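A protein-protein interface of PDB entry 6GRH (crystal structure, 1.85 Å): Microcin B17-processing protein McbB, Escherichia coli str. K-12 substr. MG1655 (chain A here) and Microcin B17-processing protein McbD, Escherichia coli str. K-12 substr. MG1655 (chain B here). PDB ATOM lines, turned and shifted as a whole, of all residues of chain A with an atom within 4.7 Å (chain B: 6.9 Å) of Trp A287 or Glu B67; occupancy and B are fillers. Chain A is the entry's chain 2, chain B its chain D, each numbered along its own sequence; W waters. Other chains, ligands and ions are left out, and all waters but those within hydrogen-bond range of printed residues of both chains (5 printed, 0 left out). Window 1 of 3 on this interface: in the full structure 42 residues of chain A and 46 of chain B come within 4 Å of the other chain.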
ATOM      1  N   PHE A 194      11.581  14.282 -23.195  1.00  0.00           N
ATOM      2  CA  PHE A 194      11.127  15.652 -22.962  1.00  0.00           C
ATOM      3  C   PHE A 194      10.782  15.969 -21.517  1.00  0.00           C
ATOM      4  O   PHE A 194      10.908  17.117 -21.109  1.00  0.00           O
ATOM      5  CB  PHE A 194       9.994  16.025 -23.925  1.00  0.00           C
ATOM      6  CG  PHE A 194      10.428  15.980 -25.350  1.00  0.00           C
ATOM      7  CD1 PHE A 194      11.171  17.014 -25.878  1.00  0.00           C
ATOM      8  CD2 PHE A 194      10.165  14.874 -26.141  1.00  0.00           C
ATOM      9  CE1 PHE A 194      11.636  16.970 -27.180  1.00  0.00           C
ATOM     10  CE2 PHE A 194      10.622  14.819 -27.445  1.00  0.00           C
ATOM     11  CZ  PHE A 194      11.344  15.873 -27.976  1.00  0.00           C
ATOM     12  N   CYS A 195      10.398  14.950 -20.750  1.00  0.00           N
ATOM     13  CA  CYS A 195      10.229  15.082 -19.296  1.00  0.00           C
ATOM     14  C   CYS A 195      11.484  15.620 -18.623  1.00  0.00           C
ATOM     15  O   CYS A 195      11.402  16.298 -17.611  1.00  0.00           O
ATOM     16  CB  CYS A 195       9.889  13.731 -18.673  1.00  0.00           C
ATOM     17  SG  CYS A 195       8.218  13.085 -18.939  1.00  0.00           S
ATOM     18  N   GLU A 198      12.733  19.466 -21.678  1.00  0.00           N
ATOM     19  CA  GLU A 198      11.793  20.586 -21.766  1.00  0.00           C
ATOM     20  C   GLU A 198      11.489  21.131 -20.385  1.00  0.00           C
ATOM     21  O   GLU A 198      11.342  22.352 -20.222  1.00  0.00           O
ATOM     22  CB  GLU A 198      10.501  20.207 -22.496  1.00  0.00           C
ATOM     23  CG  GLU A 198      10.744  19.854 -23.959  1.00  0.00           C
ATOM     24  CD  GLU A 198      11.324  21.001 -24.793  1.00  0.00           C
ATOM     25  OE1 GLU A 198      10.873  22.151 -24.588  1.00  0.00           O
ATOM     26  OE2 GLU A 198      12.255  20.757 -25.640  1.00  0.00           O
ATOM     27  N   ARG A 199      11.435  20.235 -19.390  1.00  0.00           N
ATOM     28  CA  ARG A 199      11.315  20.674 -18.000  1.00  0.00           C
ATOM     29  C   ARG A 199      12.550  21.497 -17.574  1.00  0.00           C
ATOM     30  O   ARG A 199      12.429  22.503 -16.881  1.00  0.00           O
ATOM     31  CB  ARG A 199      11.143  19.476 -17.095  1.00  0.00           C
ATOM     32  CG  ARG A 199      10.966  19.811 -15.629  1.00  0.00           C
ATOM     33  CD  ARG A 199      10.830  18.545 -14.811  1.00  0.00           C
ATOM     34  NE  ARG A 199      10.302  18.870 -13.489  1.00  0.00           N
ATOM     35  CZ  ARG A 199       9.591  18.055 -12.729  1.00  0.00           C
ATOM     36  NH1 ARG A 199       9.343  16.804 -13.115  1.00  0.00           N
ATOM     37  NH2 ARG A 199       9.144  18.490 -11.553  1.00  0.00           N
ATOM     38  N   SER A 202      12.256  24.837 -19.210  1.00  0.00           N
ATOM     39  CA  SER A 202      11.187  25.559 -18.483  1.00  0.00           C
ATOM     40  C   SER A 202      11.769  26.256 -17.256  1.00  0.00           C
ATOM     41  O   SER A 202      11.527  27.442 -17.035  1.00  0.00           O
ATOM     42  CB  SER A 202      10.074  24.576 -18.054  1.00  0.00           C
ATOM     43  OG  SER A 202       9.054  25.208 -17.280  1.00  0.00           O
ATOM     44  N   ILE A 285      12.120  11.416 -13.350  1.00  0.00           N
ATOM     45  CA  ILE A 285      10.734  11.485 -12.924  1.00  0.00           C
ATOM     46  C   ILE A 285       9.892  12.105 -14.040  1.00  0.00           C
ATOM     47  O   ILE A 285      10.417  12.679 -15.010  1.00  0.00           O
ATOM     48  CB  ILE A 285      10.605  12.254 -11.594  1.00  0.00           C
ATOM     49  CG1 ILE A 285      10.894  13.748 -11.744  1.00  0.00           C
ATOM     50  CG2 ILE A 285      11.582  11.693 -10.587  1.00  0.00           C
ATOM     51  CD1 ILE A 285      10.543  14.562 -10.518  1.00  0.00           C
ATOM     52  N   HIS A 286       8.584  11.914 -13.937  1.00  0.00           N
ATOM     53  CA  HIS A 286       7.659  12.497 -14.894  1.00  0.00           C
ATOM     54  C   HIS A 286       7.574  13.999 -14.652  1.00  0.00           C
ATOM     55  O   HIS A 286       7.766  14.453 -13.517  1.00  0.00           O
ATOM     56  CB  HIS A 286       6.265  11.900 -14.769  1.00  0.00           C
ATOM     57  CG  HIS A 286       5.985  10.783 -15.712  1.00  0.00           C
ATOM     58  ND1 HIS A 286       5.971  10.959 -17.081  1.00  0.00           N
ATOM     59  CD2 HIS A 286       5.645   9.495 -15.501  1.00  0.00           C
ATOM     60  CE1 HIS A 286       5.655   9.819 -17.663  1.00  0.00           C
ATOM     61  NE2 HIS A 286       5.446   8.917 -16.731  1.00  0.00           N
ATOM     62  N   TRP A 287       7.338  14.734 -15.738  1.00  0.00           N
ATOM     63  CA  TRP A 287       6.941  16.134 -15.702  1.00  0.00           C
ATOM     64  C   TRP A 287       5.424  16.228 -16.006  1.00  0.00           C
ATOM     65  O   TRP A 287       4.976  15.824 -17.080  1.00  0.00           O
ATOM     66  CB  TRP A 287       7.738  16.933 -16.737  1.00  0.00           C
ATOM     67  CG  TRP A 287       7.523  18.414 -16.683  1.00  0.00           C
ATOM     68  CD1 TRP A 287       7.258  19.186 -15.573  1.00  0.00           C
ATOM     69  CD2 TRP A 287       7.602  19.305 -17.780  1.00  0.00           C
ATOM     70  NE1 TRP A 287       7.145  20.498 -15.932  1.00  0.00           N
ATOM     71  CE2 TRP A 287       7.381  20.606 -17.279  1.00  0.00           C
ATOM     72  CE3 TRP A 287       7.856  19.136 -19.147  1.00  0.00           C
ATOM     73  CZ2 TRP A 287       7.384  21.737 -18.108  1.00  0.00           C
ATOM     74  CZ3 TRP A 287       7.862  20.260 -19.974  1.00  0.00           C
ATOM     75  CH2 TRP A 287       7.614  21.546 -19.449  1.00  0.00           C
ATOM     76  N   GLN A 288       4.642  16.744 -15.057  1.00  0.00           N
ATOM     77  CA  GLN A 288       3.173  16.834 -15.207  1.00  0.00           C
ATOM     78  C   GLN A 288       2.737  17.526 -16.535  1.00  0.00           C
ATOM     79  O   GLN A 288       1.740  17.143 -17.136  1.00  0.00           O
ATOM     80  CB  GLN A 288       2.549  17.542 -13.983  1.00  0.00           C
ATOM     81  CG  GLN A 288       1.080  17.975 -14.116  1.00  0.00           C
ATOM     82  CD  GLN A 288       0.089  16.806 -14.015  1.00  0.00           C
ATOM     83  OE1 GLN A 288      -0.535  16.580 -12.949  1.00  0.00           O
ATOM     84  NE2 GLN A 288      -0.029  16.027 -15.106  1.00  0.00           N
ATOM     85  N   ALA A 289       3.516  18.508 -16.985  1.00  0.00           N
ATOM     86  CA  ALA A 289       3.211  19.259 -18.200  1.00  0.00           C
ATOM     87  C   ALA A 289       3.576  18.544 -19.507  1.00  0.00           C
ATOM     88  O   ALA A 289       3.260  19.046 -20.571  1.00  0.00           O
ATOM     89  CB  ALA A 289       3.913  20.608 -18.158  1.00  0.00           C
ATOM     90  N   CYS A 290       4.246  17.398 -19.452  1.00  0.00           N
ATOM     91  CA  CYS A 290       4.734  16.781 -20.686  1.00  0.00           C
ATOM     92  C   CYS A 290       3.624  16.193 -21.540  1.00  0.00           C
ATOM     93  O   CYS A 290       2.617  15.682 -21.040  1.00  0.00           O
ATOM     94  CB  CYS A 290       5.770  15.699 -20.392  1.00  0.00           C
ATOM     95  SG  CYS A 290       6.675  15.187 -21.873  1.00  0.00           S
ATOM     96  N   LEU A 293       2.178  12.539 -21.280  1.00  0.00           N
ATOM     97  CA  LEU A 293       1.039  12.245 -20.387  1.00  0.00           C
ATOM     98  C   LEU A 293      -0.342  12.543 -20.995  1.00  0.00           C
ATOM     99  O   LEU A 293      -1.347  12.262 -20.356  1.00  0.00           O
ATOM    100  CB  LEU A 293       1.210  12.977 -19.050  1.00  0.00           C
ATOM    101  CG  LEU A 293       2.416  12.492 -18.244  1.00  0.00           C
ATOM    102  CD1 LEU A 293       2.693  13.405 -17.059  1.00  0.00           C
ATOM    103  CD2 LEU A 293       2.233  11.058 -17.767  1.00  0.00           C
ATOM    104  N   ALA B  11      18.789  17.469 -13.983  1.00  0.00           N
ATOM    105  CA  ALA B  11      17.431  17.726 -13.564  1.00  0.00           C
ATOM    106  C   ALA B  11      17.381  18.227 -12.120  1.00  0.00           C
ATOM    107  O   ALA B  11      16.436  18.939 -11.765  1.00  0.00           O
ATOM    108  CB  ALA B  11      16.584  16.456 -13.681  1.00  0.00           C
ATOM    109  N   TYR B  58      11.667  22.490  -1.749  1.00  0.00           N
ATOM    110  CA  TYR B  58      12.252  22.626  -3.061  1.00  0.00           C
ATOM    111  C   TYR B  58      11.284  22.168  -4.166  1.00  0.00           C
ATOM    112  O   TYR B  58      11.084  22.900  -5.133  1.00  0.00           O
ATOM    113  CB  TYR B  58      13.570  21.821  -3.170  1.00  0.00           C
ATOM    114  CG  TYR B  58      14.090  21.838  -4.569  1.00  0.00           C
ATOM    115  CD1 TYR B  58      14.682  22.971  -5.065  1.00  0.00           C
ATOM    116  CD2 TYR B  58      13.957  20.742  -5.404  1.00  0.00           C
ATOM    117  CE1 TYR B  58      15.155  23.029  -6.366  1.00  0.00           C
ATOM    118  CE2 TYR B  58      14.424  20.794  -6.725  1.00  0.00           C
ATOM    119  CZ  TYR B  58      15.006  21.937  -7.190  1.00  0.00           C
ATOM    120  OH  TYR B  58      15.489  22.000  -8.461  1.00  0.00           O
ATOM    121  N   PHE B  59      10.724  20.965  -4.044  1.00  0.00           N
ATOM    122  CA  PHE B  59       9.791  20.468  -5.056  1.00  0.00           C
ATOM    123  C   PHE B  59       8.589  21.420  -5.197  1.00  0.00           C
ATOM    124  O   PHE B  59       8.163  21.720  -6.317  1.00  0.00           O
ATOM    125  CB  PHE B  59       9.262  19.080  -4.729  1.00  0.00           C
ATOM    126  CG  PHE B  59      10.042  17.951  -5.332  1.00  0.00           C
ATOM    127  CD1 PHE B  59       9.650  17.403  -6.556  1.00  0.00           C
ATOM    128  CD2 PHE B  59      11.107  17.360  -4.651  1.00  0.00           C
ATOM    129  CE1 PHE B  59      10.342  16.325  -7.117  1.00  0.00           C
ATOM    130  CE2 PHE B  59      11.807  16.273  -5.197  1.00  0.00           C
ATOM    131  CZ  PHE B  59      11.416  15.742  -6.424  1.00  0.00           C
ATOM    132  N   GLU B  60       8.067  21.880  -4.061  1.00  0.00           N
ATOM    133  CA  GLU B  60       6.915  22.790  -4.051  1.00  0.00           C
ATOM    134  C   GLU B  60       7.214  24.095  -4.800  1.00  0.00           C
ATOM    135  O   GLU B  60       6.506  24.459  -5.711  1.00  0.00           O
ATOM    136  CB  GLU B  60       6.514  23.143  -2.618  1.00  0.00           C
ATOM    137  CG  GLU B  60       5.323  24.077  -2.542  1.00  0.00           C
ATOM    138  CD  GLU B  60       5.243  24.824  -1.219  1.00  0.00           C
ATOM    139  OE1 GLU B  60       5.358  24.152  -0.182  1.00  0.00           O
ATOM    140  OE2 GLU B  60       5.059  26.074  -1.236  1.00  0.00           O
ATOM    141  N   ARG B  61       8.254  24.787  -4.372  1.00  0.00           N
ATOM    142  CA  ARG B  61       8.621  26.070  -4.950  1.00  0.00           C
ATOM    143  C   ARG B  61       9.043  25.974  -6.398  1.00  0.00           C
ATOM    144  O   ARG B  61       8.682  26.843  -7.208  1.00  0.00           O
ATOM    145  CB  ARG B  61       9.692  26.756  -4.100  1.00  0.00           C
ATOM    146  CG  ARG B  61       9.147  27.050  -2.704  1.00  0.00           C
ATOM    147  CD  ARG B  61       9.421  28.458  -2.226  1.00  0.00           C
ATOM    148  NE  ARG B  61      10.838  28.592  -1.991  1.00  0.00           N
ATOM    149  CZ  ARG B  61      11.431  28.649  -0.803  1.00  0.00           C
ATOM    150  NH1 ARG B  61      10.748  28.614   0.344  1.00  0.00           N
ATOM    151  NH2 ARG B  61      12.741  28.787  -0.771  1.00  0.00           N
ATOM    152  N   ARG B  62       9.764  24.917  -6.747  1.00  0.00           N
ATOM    153  CA  ARG B  62      10.112  24.707  -8.139  1.00  0.00           C
ATOM    154  C   ARG B  62       8.866  24.533  -9.009  1.00  0.00           C
ATOM    155  O   ARG B  62       8.786  25.078 -10.120  1.00  0.00           O
ATOM    156  CB  ARG B  62      11.054  23.521  -8.322  1.00  0.00           C
ATOM    157  CG  ARG B  62      11.501  23.367  -9.769  1.00  0.00           C
ATOM    158  CD  ARG B  62      12.487  22.216  -9.920  1.00  0.00           C
ATOM    159  NE  ARG B  62      11.904  20.901  -9.606  1.00  0.00           N
ATOM    160  CZ  ARG B  62      12.498  19.733  -9.870  1.00  0.00           C
ATOM    161  NH1 ARG B  62      13.707  19.653 -10.449  1.00  0.00           N
ATOM    162  NH2 ARG B  62      11.875  18.628  -9.590  1.00  0.00           N
ATOM    163  N   HIS B  63       7.889  23.797  -8.503  1.00  0.00           N
ATOM    164  CA  HIS B  63       6.670  23.588  -9.263  1.00  0.00           C
ATOM    165  C   HIS B  63       5.912  24.908  -9.578  1.00  0.00           C
ATOM    166  O   HIS B  63       5.601  25.212 -10.742  1.00  0.00           O
ATOM    167  CB  HIS B  63       5.733  22.643  -8.524  1.00  0.00           C
ATOM    168  CG  HIS B  63       4.472  22.371  -9.276  1.00  0.00           C
ATOM    169  ND1 HIS B  63       4.421  21.505 -10.348  1.00  0.00           N
ATOM    170  CD2 HIS B  63       3.215  22.845  -9.104  1.00  0.00           C
ATOM    171  CE1 HIS B  63       3.176  21.444 -10.791  1.00  0.00           C
ATOM    172  NE2 HIS B  63       2.424  22.246 -10.054  1.00  0.00           N
ATOM    173  N   PHE B  64       5.619  25.658  -8.523  1.00  0.00           N
ATOM    174  CA  PHE B  64       4.797  26.874  -8.623  1.00  0.00           C
ATOM    175  C   PHE B  64       5.544  28.027  -9.289  1.00  0.00           C
ATOM    176  O   PHE B  64       4.938  28.770 -10.072  1.00  0.00           O
ATOM    177  CB  PHE B  64       4.215  27.254  -7.258  1.00  0.00           C
ATOM    178  CG  PHE B  64       3.178  26.287  -6.784  1.00  0.00           C
ATOM    179  CD1 PHE B  64       1.893  26.324  -7.324  1.00  0.00           C
ATOM    180  CD2 PHE B  64       3.464  25.324  -5.822  1.00  0.00           C
ATOM    181  CE1 PHE B  64       0.922  25.427  -6.899  1.00  0.00           C
ATOM    182  CE2 PHE B  64       2.495  24.426  -5.404  1.00  0.00           C
ATOM    183  CZ  PHE B  64       1.228  24.471  -5.954  1.00  0.00           C
ATOM    184  N   PHE B  65       6.850  28.132  -9.054  1.00  0.00           N
ATOM    185  CA  PHE B  65       7.681  29.191  -9.683  1.00  0.00           C
ATOM    186  C   PHE B  65       8.155  28.890 -11.105  1.00  0.00           C
ATOM    187  O   PHE B  65       8.294  29.808 -11.929  1.00  0.00           O
ATOM    188  CB  PHE B  65       8.909  29.523  -8.810  1.00  0.00           C
ATOM    189  CG  PHE B  65       8.615  30.433  -7.654  1.00  0.00           C
ATOM    190  CD1 PHE B  65       8.057  29.945  -6.473  1.00  0.00           C
ATOM    191  CD2 PHE B  65       8.903  31.788  -7.745  1.00  0.00           C
ATOM    192  CE1 PHE B  65       7.789  30.790  -5.417  1.00  0.00           C
ATOM    193  CE2 PHE B  65       8.609  32.647  -6.691  1.00  0.00           C
ATOM    194  CZ  PHE B  65       8.055  32.153  -5.537  1.00  0.00           C
ATOM    195  N   ASN B  66       8.430  27.628 -11.417  1.00  0.00           N
ATOM    196  CA  ASN B  66       9.225  27.330 -12.626  1.00  0.00           C
ATOM    197  C   ASN B  66       8.571  26.401 -13.608  1.00  0.00           C
ATOM    198  O   ASN B  66       9.110  26.268 -14.726  1.00  0.00           O
ATOM    199  CB  ASN B  66      10.542  26.637 -12.284  1.00  0.00           C
ATOM    200  CG  ASN B  66      11.457  27.437 -11.393  1.00  0.00           C
ATOM    201  OD1 ASN B  66      12.252  26.829 -10.679  1.00  0.00           O
ATOM    202  ND2 ASN B  66      11.382  28.760 -11.420  1.00  0.00           N
ATOM    203  N   GLU B  67       7.501  25.708 -13.219  1.00  0.00           N
ATOM    204  CA  GLU B  67       7.094  24.491 -13.946  1.00  0.00           C
ATOM    205  C   GLU B  67       5.632  24.349 -14.374  1.00  0.00           C
ATOM    206  O   GLU B  67       5.299  23.314 -14.981  1.00  0.00           O
ATOM    207  CB  GLU B  67       7.479  23.265 -13.131  1.00  0.00           C
ATOM    208  CG  GLU B  67       8.977  23.054 -12.992  1.00  0.00           C
ATOM    209  CD  GLU B  67       9.316  21.799 -12.194  1.00  0.00           C
ATOM    210  OE1 GLU B  67       8.437  21.247 -11.475  1.00  0.00           O
ATOM    211  OE2 GLU B  67      10.483  21.353 -12.244  1.00  0.00           O
ATOM    212  N   ILE B  68       4.785  25.356 -14.132  1.00  0.00           N
ATOM    213  CA  ILE B  68       3.371  25.225 -14.473  1.00  0.00           C
ATOM    214  C   ILE B  68       3.180  25.432 -15.980  1.00  0.00           C
ATOM    215  O   ILE B  68       3.687  26.409 -16.534  1.00  0.00           O
ATOM    216  CB  ILE B  68       2.460  26.253 -13.760  1.00  0.00           C
ATOM    217  CG1 ILE B  68       2.712  26.330 -12.242  1.00  0.00           C
ATOM    218  CG2 ILE B  68       0.981  25.955 -14.057  1.00  0.00           C
ATOM    219  CD1 ILE B  68       1.972  25.324 -11.400  1.00  0.00           C
ATOM    220  N   VAL B  69       2.439  24.518 -16.616  1.00  0.00           N
ATOM    221  CA  VAL B  69       1.921  24.724 -17.975  1.00  0.00           C
ATOM    222  C   VAL B  69       0.403  24.634 -17.892  1.00  0.00           C
ATOM    223  O   VAL B  69      -0.137  23.692 -17.310  1.00  0.00           O
ATOM    224  CB  VAL B  69       2.494  23.717 -19.001  1.00  0.00           C
ATOM    225  CG1 VAL B  69       1.850  23.898 -20.383  1.00  0.00           C
ATOM    226  CG2 VAL B  69       4.019  23.886 -19.107  1.00  0.00           C
ATOM    227  N   ASP B 132       5.566  32.566 -11.801  1.00  0.00           N
ATOM    228  CA  ASP B 132       6.340  33.220 -12.870  1.00  0.00           C
ATOM    229  C   ASP B 132       5.466  34.187 -13.692  1.00  0.00           C
ATOM    230  O   ASP B 132       4.241  34.133 -13.620  1.00  0.00           O
ATOM    231  CB  ASP B 132       6.931  32.170 -13.803  1.00  0.00           C
ATOM    232  CG  ASP B 132       5.876  31.507 -14.659  1.00  0.00           C
ATOM    233  OD1 ASP B 132       5.091  30.690 -14.118  1.00  0.00           O
ATOM    234  OD2 ASP B 132       5.795  31.834 -15.866  1.00  0.00           O
ATOM    235  N   THR B 135       3.657  32.232 -17.603  1.00  0.00           N
ATOM    236  CA  THR B 135       2.610  31.221 -17.683  1.00  0.00           C
ATOM    237  C   THR B 135       1.250  31.822 -18.043  1.00  0.00           C
ATOM    238  O   THR B 135       0.607  31.354 -18.976  1.00  0.00           O
ATOM    239  CB  THR B 135       2.544  30.437 -16.370  1.00  0.00           C
ATOM    240  OG1 THR B 135       3.823  29.837 -16.145  1.00  0.00           O
ATOM    241  CG2 THR B 135       1.495  29.367 -16.433  1.00  0.00           C
ATOM    242  N   TYR B 341      -6.300  23.134  -6.314  1.00  0.00           N
ATOM    243  CA  TYR B 341      -5.441  22.902  -7.457  1.00  0.00           C
ATOM    244  C   TYR B 341      -4.588  21.709  -7.137  1.00  0.00           C
ATOM    245  O   TYR B 341      -4.100  21.569  -5.996  1.00  0.00           O
ATOM    246  CB  TYR B 341      -4.518  24.088  -7.735  1.00  0.00           C
ATOM    247  CG  TYR B 341      -3.344  23.718  -8.593  1.00  0.00           C
ATOM    248  CD1 TYR B 341      -3.480  23.587  -9.962  1.00  0.00           C
ATOM    249  CD2 TYR B 341      -2.099  23.493  -8.031  1.00  0.00           C
ATOM    250  CE1 TYR B 341      -2.404  23.260 -10.763  1.00  0.00           C
ATOM    251  CE2 TYR B 341      -1.004  23.121  -8.809  1.00  0.00           C
ATOM    252  CZ  TYR B 341      -1.152  23.012 -10.178  1.00  0.00           C
ATOM    253  OH  TYR B 341      -0.067  22.649 -10.949  1.00  0.00           O
ATOM    254  N   ARG B 344       0.413  16.076 -10.182  1.00  0.00           N
ATOM    255  CA  ARG B 344       1.129  14.902  -9.723  1.00  0.00           C
ATOM    256  C   ARG B 344       2.103  14.379 -10.763  1.00  0.00           C
ATOM    257  O   ARG B 344       1.923  14.568 -11.974  1.00  0.00           O
ATOM    258  CB  ARG B 344       0.186  13.821  -9.215  1.00  0.00           C
ATOM    259  CG  ARG B 344      -0.569  13.034 -10.274  1.00  0.00           C
ATOM    260  CD  ARG B 344      -1.348  13.923 -11.209  1.00  0.00           C
ATOM    261  NE  ARG B 344      -2.400  13.209 -11.923  1.00  0.00           N
ATOM    262  CZ  ARG B 344      -3.214  13.769 -12.821  1.00  0.00           C
ATOM    263  NH1 ARG B 344      -3.066  15.048 -13.161  1.00  0.00           N
ATOM    264  NH2 ARG B 344      -4.179  13.037 -13.398  1.00  0.00           N
ATOM    265  N   GLU B 345       3.148  13.722 -10.257  1.00  0.00           N
ATOM    266  CA  GLU B 345       4.251  13.212 -11.087  1.00  0.00           C
ATOM    267  C   GLU B 345       4.745  11.877 -10.526  1.00  0.00           C
ATOM    268  O   GLU B 345       4.955  11.738  -9.315  1.00  0.00           O
ATOM    269  CB  GLU B 345       5.418  14.228 -11.107  1.00  0.00           C
ATOM    270  CG  GLU B 345       5.040  15.549 -11.755  1.00  0.00           C
ATOM    271  CD  GLU B 345       6.119  16.621 -11.726  1.00  0.00           C
ATOM    272  OE1 GLU B 345       7.005  16.612 -10.810  1.00  0.00           O
ATOM    273  OE2 GLU B 345       6.050  17.488 -12.634  1.00  0.00           O
ATOM    274  N   ARG B 346       4.907  10.904 -11.402  1.00  0.00           N
ATOM    275  CA  ARG B 346       5.481   9.639 -11.041  1.00  0.00           C
ATOM    276  C   ARG B 346       6.959   9.748 -10.656  1.00  0.00           C
ATOM    277  O   ARG B 346       7.779  10.337 -11.387  1.00  0.00           O
ATOM    278  CB  ARG B 346       5.285   8.645 -12.159  1.00  0.00           C
ATOM    279  CG  ARG B 346       5.491   7.221 -11.736  1.00  0.00           C
ATOM    280  CD  ARG B 346       5.192   6.239 -12.856  1.00  0.00           C
ATOM    281  NE  ARG B 346       5.561   4.891 -12.453  1.00  0.00           N
ATOM    282  CZ  ARG B 346       5.456   3.802 -13.212  1.00  0.00           C
ATOM    283  NH1 ARG B 346       5.029   3.866 -14.467  1.00  0.00           N
ATOM    284  NH2 ARG B 346       5.816   2.624 -12.705  1.00  0.00           N
ATOM    285  N   TYR B 354       1.430  17.990  -5.777  1.00  0.00           N
ATOM    286  CA  TYR B 354       1.501  19.426  -5.539  1.00  0.00           C
ATOM    287  C   TYR B 354       0.062  19.887  -5.418  1.00  0.00           C
ATOM    288  O   TYR B 354      -0.789  19.485  -6.245  1.00  0.00           O
ATOM    289  CB  TYR B 354       2.162  20.147  -6.709  1.00  0.00           C
ATOM    290  CG  TYR B 354       3.436  19.520  -7.193  1.00  0.00           C
ATOM    291  CD1 TYR B 354       3.416  18.479  -8.111  1.00  0.00           C
ATOM    292  CD2 TYR B 354       4.674  19.981  -6.752  1.00  0.00           C
ATOM    293  CE1 TYR B 354       4.609  17.898  -8.575  1.00  0.00           C
ATOM    294  CE2 TYR B 354       5.862  19.414  -7.193  1.00  0.00           C
ATOM    295  CZ  TYR B 354       5.831  18.389  -8.114  1.00  0.00           C
ATOM    296  OH  TYR B 354       7.014  17.839  -8.564  1.00  0.00           O
HETATM  297  O   HOH W   1       6.080  20.074 -12.118  1.00  0.00           O
HETATM  298  O   HOH W   2       6.444  25.543 -17.745  1.00  0.00           O
HETATM  299  O   HOH W   3       4.444  20.884 -14.285  1.00  0.00           O
HETATM  300  O   HOH W   4      12.880  21.781 -13.525  1.00  0.00           O
HETATM  301  O   HOH W   5       9.196  20.441  -8.706  1.00  0.00           O
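Water W1 lies within hydrogen-bond range of OE2 of Glu B345 (2.6 Å), OE1 of Glu B67 (2.7 Å), ND1 of His B63 (2.8 Å) and NH2 of Arg A199 (3.5 Å).
Water W3 bridges O of Glu B67 and NE1 of Trp A287.
Water W2 lies within hydrogen-bond range of the side-chain hydroxyl of Ser A202 (2.7 Å) and the backbone carbonyl oxygen of Ile B68 (3.1 Å).
Water W4 bridges OE2 of Glu B67 and O of Arg A199.
Water W5 lies within hydrogen-bond range of the guanidinium group (NE) of Arg B62 (2.9 Å), the backbone carbonyl oxygen (O) of Phe B59 (2.9 Å), the side-chain carboxylate (OE1) of Glu B67 (3.0 Å), the side-chain hydroxyl (OH) of Tyr B354 (3.4 Å) and the guanidinium group (NH2) of Arg A199 (3.5 Å).
NE of Arg A199 is in salt-bridge range of OE2 of Glu B67 (2.8 Å).
The side-chain carboxylate (OE1) of Glu B345 lies within salt-bridge range of the guanidinium group (NH2) of Arg A199 (2.9 Å).
The side-chain hydroxyl (OG) of Ser A202 sits at hydrogen-bond distance from the backbone carbonyl oxygen (O) of Asn B66 (2.8 Å).
N of His A286 lies within hydrogen-bond range of O of Arg B346, 3.1 Å away.
O of Glu B67 is in hydrogen-bond range of NE1 of Trp A287, 3.5 Å away.
OE1 of Gln A288 is in hydrogen-bond range of NH1 of Arg B344, 3.0 Å away.
The backbone NH (N) of Gln A288 is in hydrogen-bond range of the side-chain carboxylate (OE2) of Glu B345, at 2.9 Å.
The guanidinium group of Arg B62 lies close to the guanidinium group of Arg A199 (3.4 Å).
OH of Tyr B354 touches NH2 of Arg A199, 3.7 Å away.
Ser A202 touches Glu B67.
Ile A285 touches Phe B59.
Ile A285 touches Arg B346 (CB to O, 3.4 Å).
CD of Glu B345 touches O of His A286 (3.3 Å).
OE2 of Glu B345 touches CA of Trp A287 (3.5 Å).
Ala A289 touches Val B69.
The side-chain sulfur (SG) of Cys A195 sits close to a ring nitrogen (ND1) of His A286, 3.6 Å away.
The side-chain sulfur of Cys A195 lies close to the backbone NH of Trp A287.
The backbone carbonyl oxygen (O) of His A286 is in hydrogen-bond range of the guanidinium group (NH1) of Arg A199, 2.9 Å away.
O of Ala B11 sits at hydrogen-bond distance from NH1 of Arg B62, 3.1 Å away.
The guanidinium group (NE) of Arg B62 lies within salt-bridge range of the side-chain carboxylate (OE2) of Glu B67 (3.0 Å).
OE1 of Glu B345 lies within hydrogen-bond range of OH of Tyr B354 (2.6 Å).
Hydrophobic or aromatic side chains of chain A within 4 Å of the printed part of chain B: Ile A285, His A286, Trp A287 and Ala A289.
Hydrophobic or aromatic side chains of chain B within 4 Å of the printed part of chain A: Phe B59, Val B69 and Tyr B354.
Among the printed residues, Asp or Glu carboxylates within 4 Å of a Lys or Arg side-chain nitrogen of the other chain: Arg A199 with Glu B67 (2.8 Å) and Arg A199 with Glu B345 (2.9 Å).
Trp A287 touches just these residues of chain B: Glu B67 and Glu B345.
Of chain A, only Arg A199 (2.8 Å), Ser A202 (3.9 Å) and Trp A287 (3.5 Å) come within 4 Å of Glu B67.
Of the printed residues of chain A, Glu B345 touches Arg A199 (2.9 Å), His A286 (3.3 Å), Trp A287 (3.5 Å) and Gln A288 (2.9 Å).
Of the printed residues of chain B, Arg A199 touches Arg B62, Glu B67, Glu B345 and Tyr B354.
Of the printed residues of chain A, Tyr B354 touches Arg A199.
The nearest residue of chain A that does not touch Glu B67 is Ala A289 (4.4 Å).
The nearest printed residue of chain A that does not touch Phe B59 is Arg A199 (5.1 Å).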
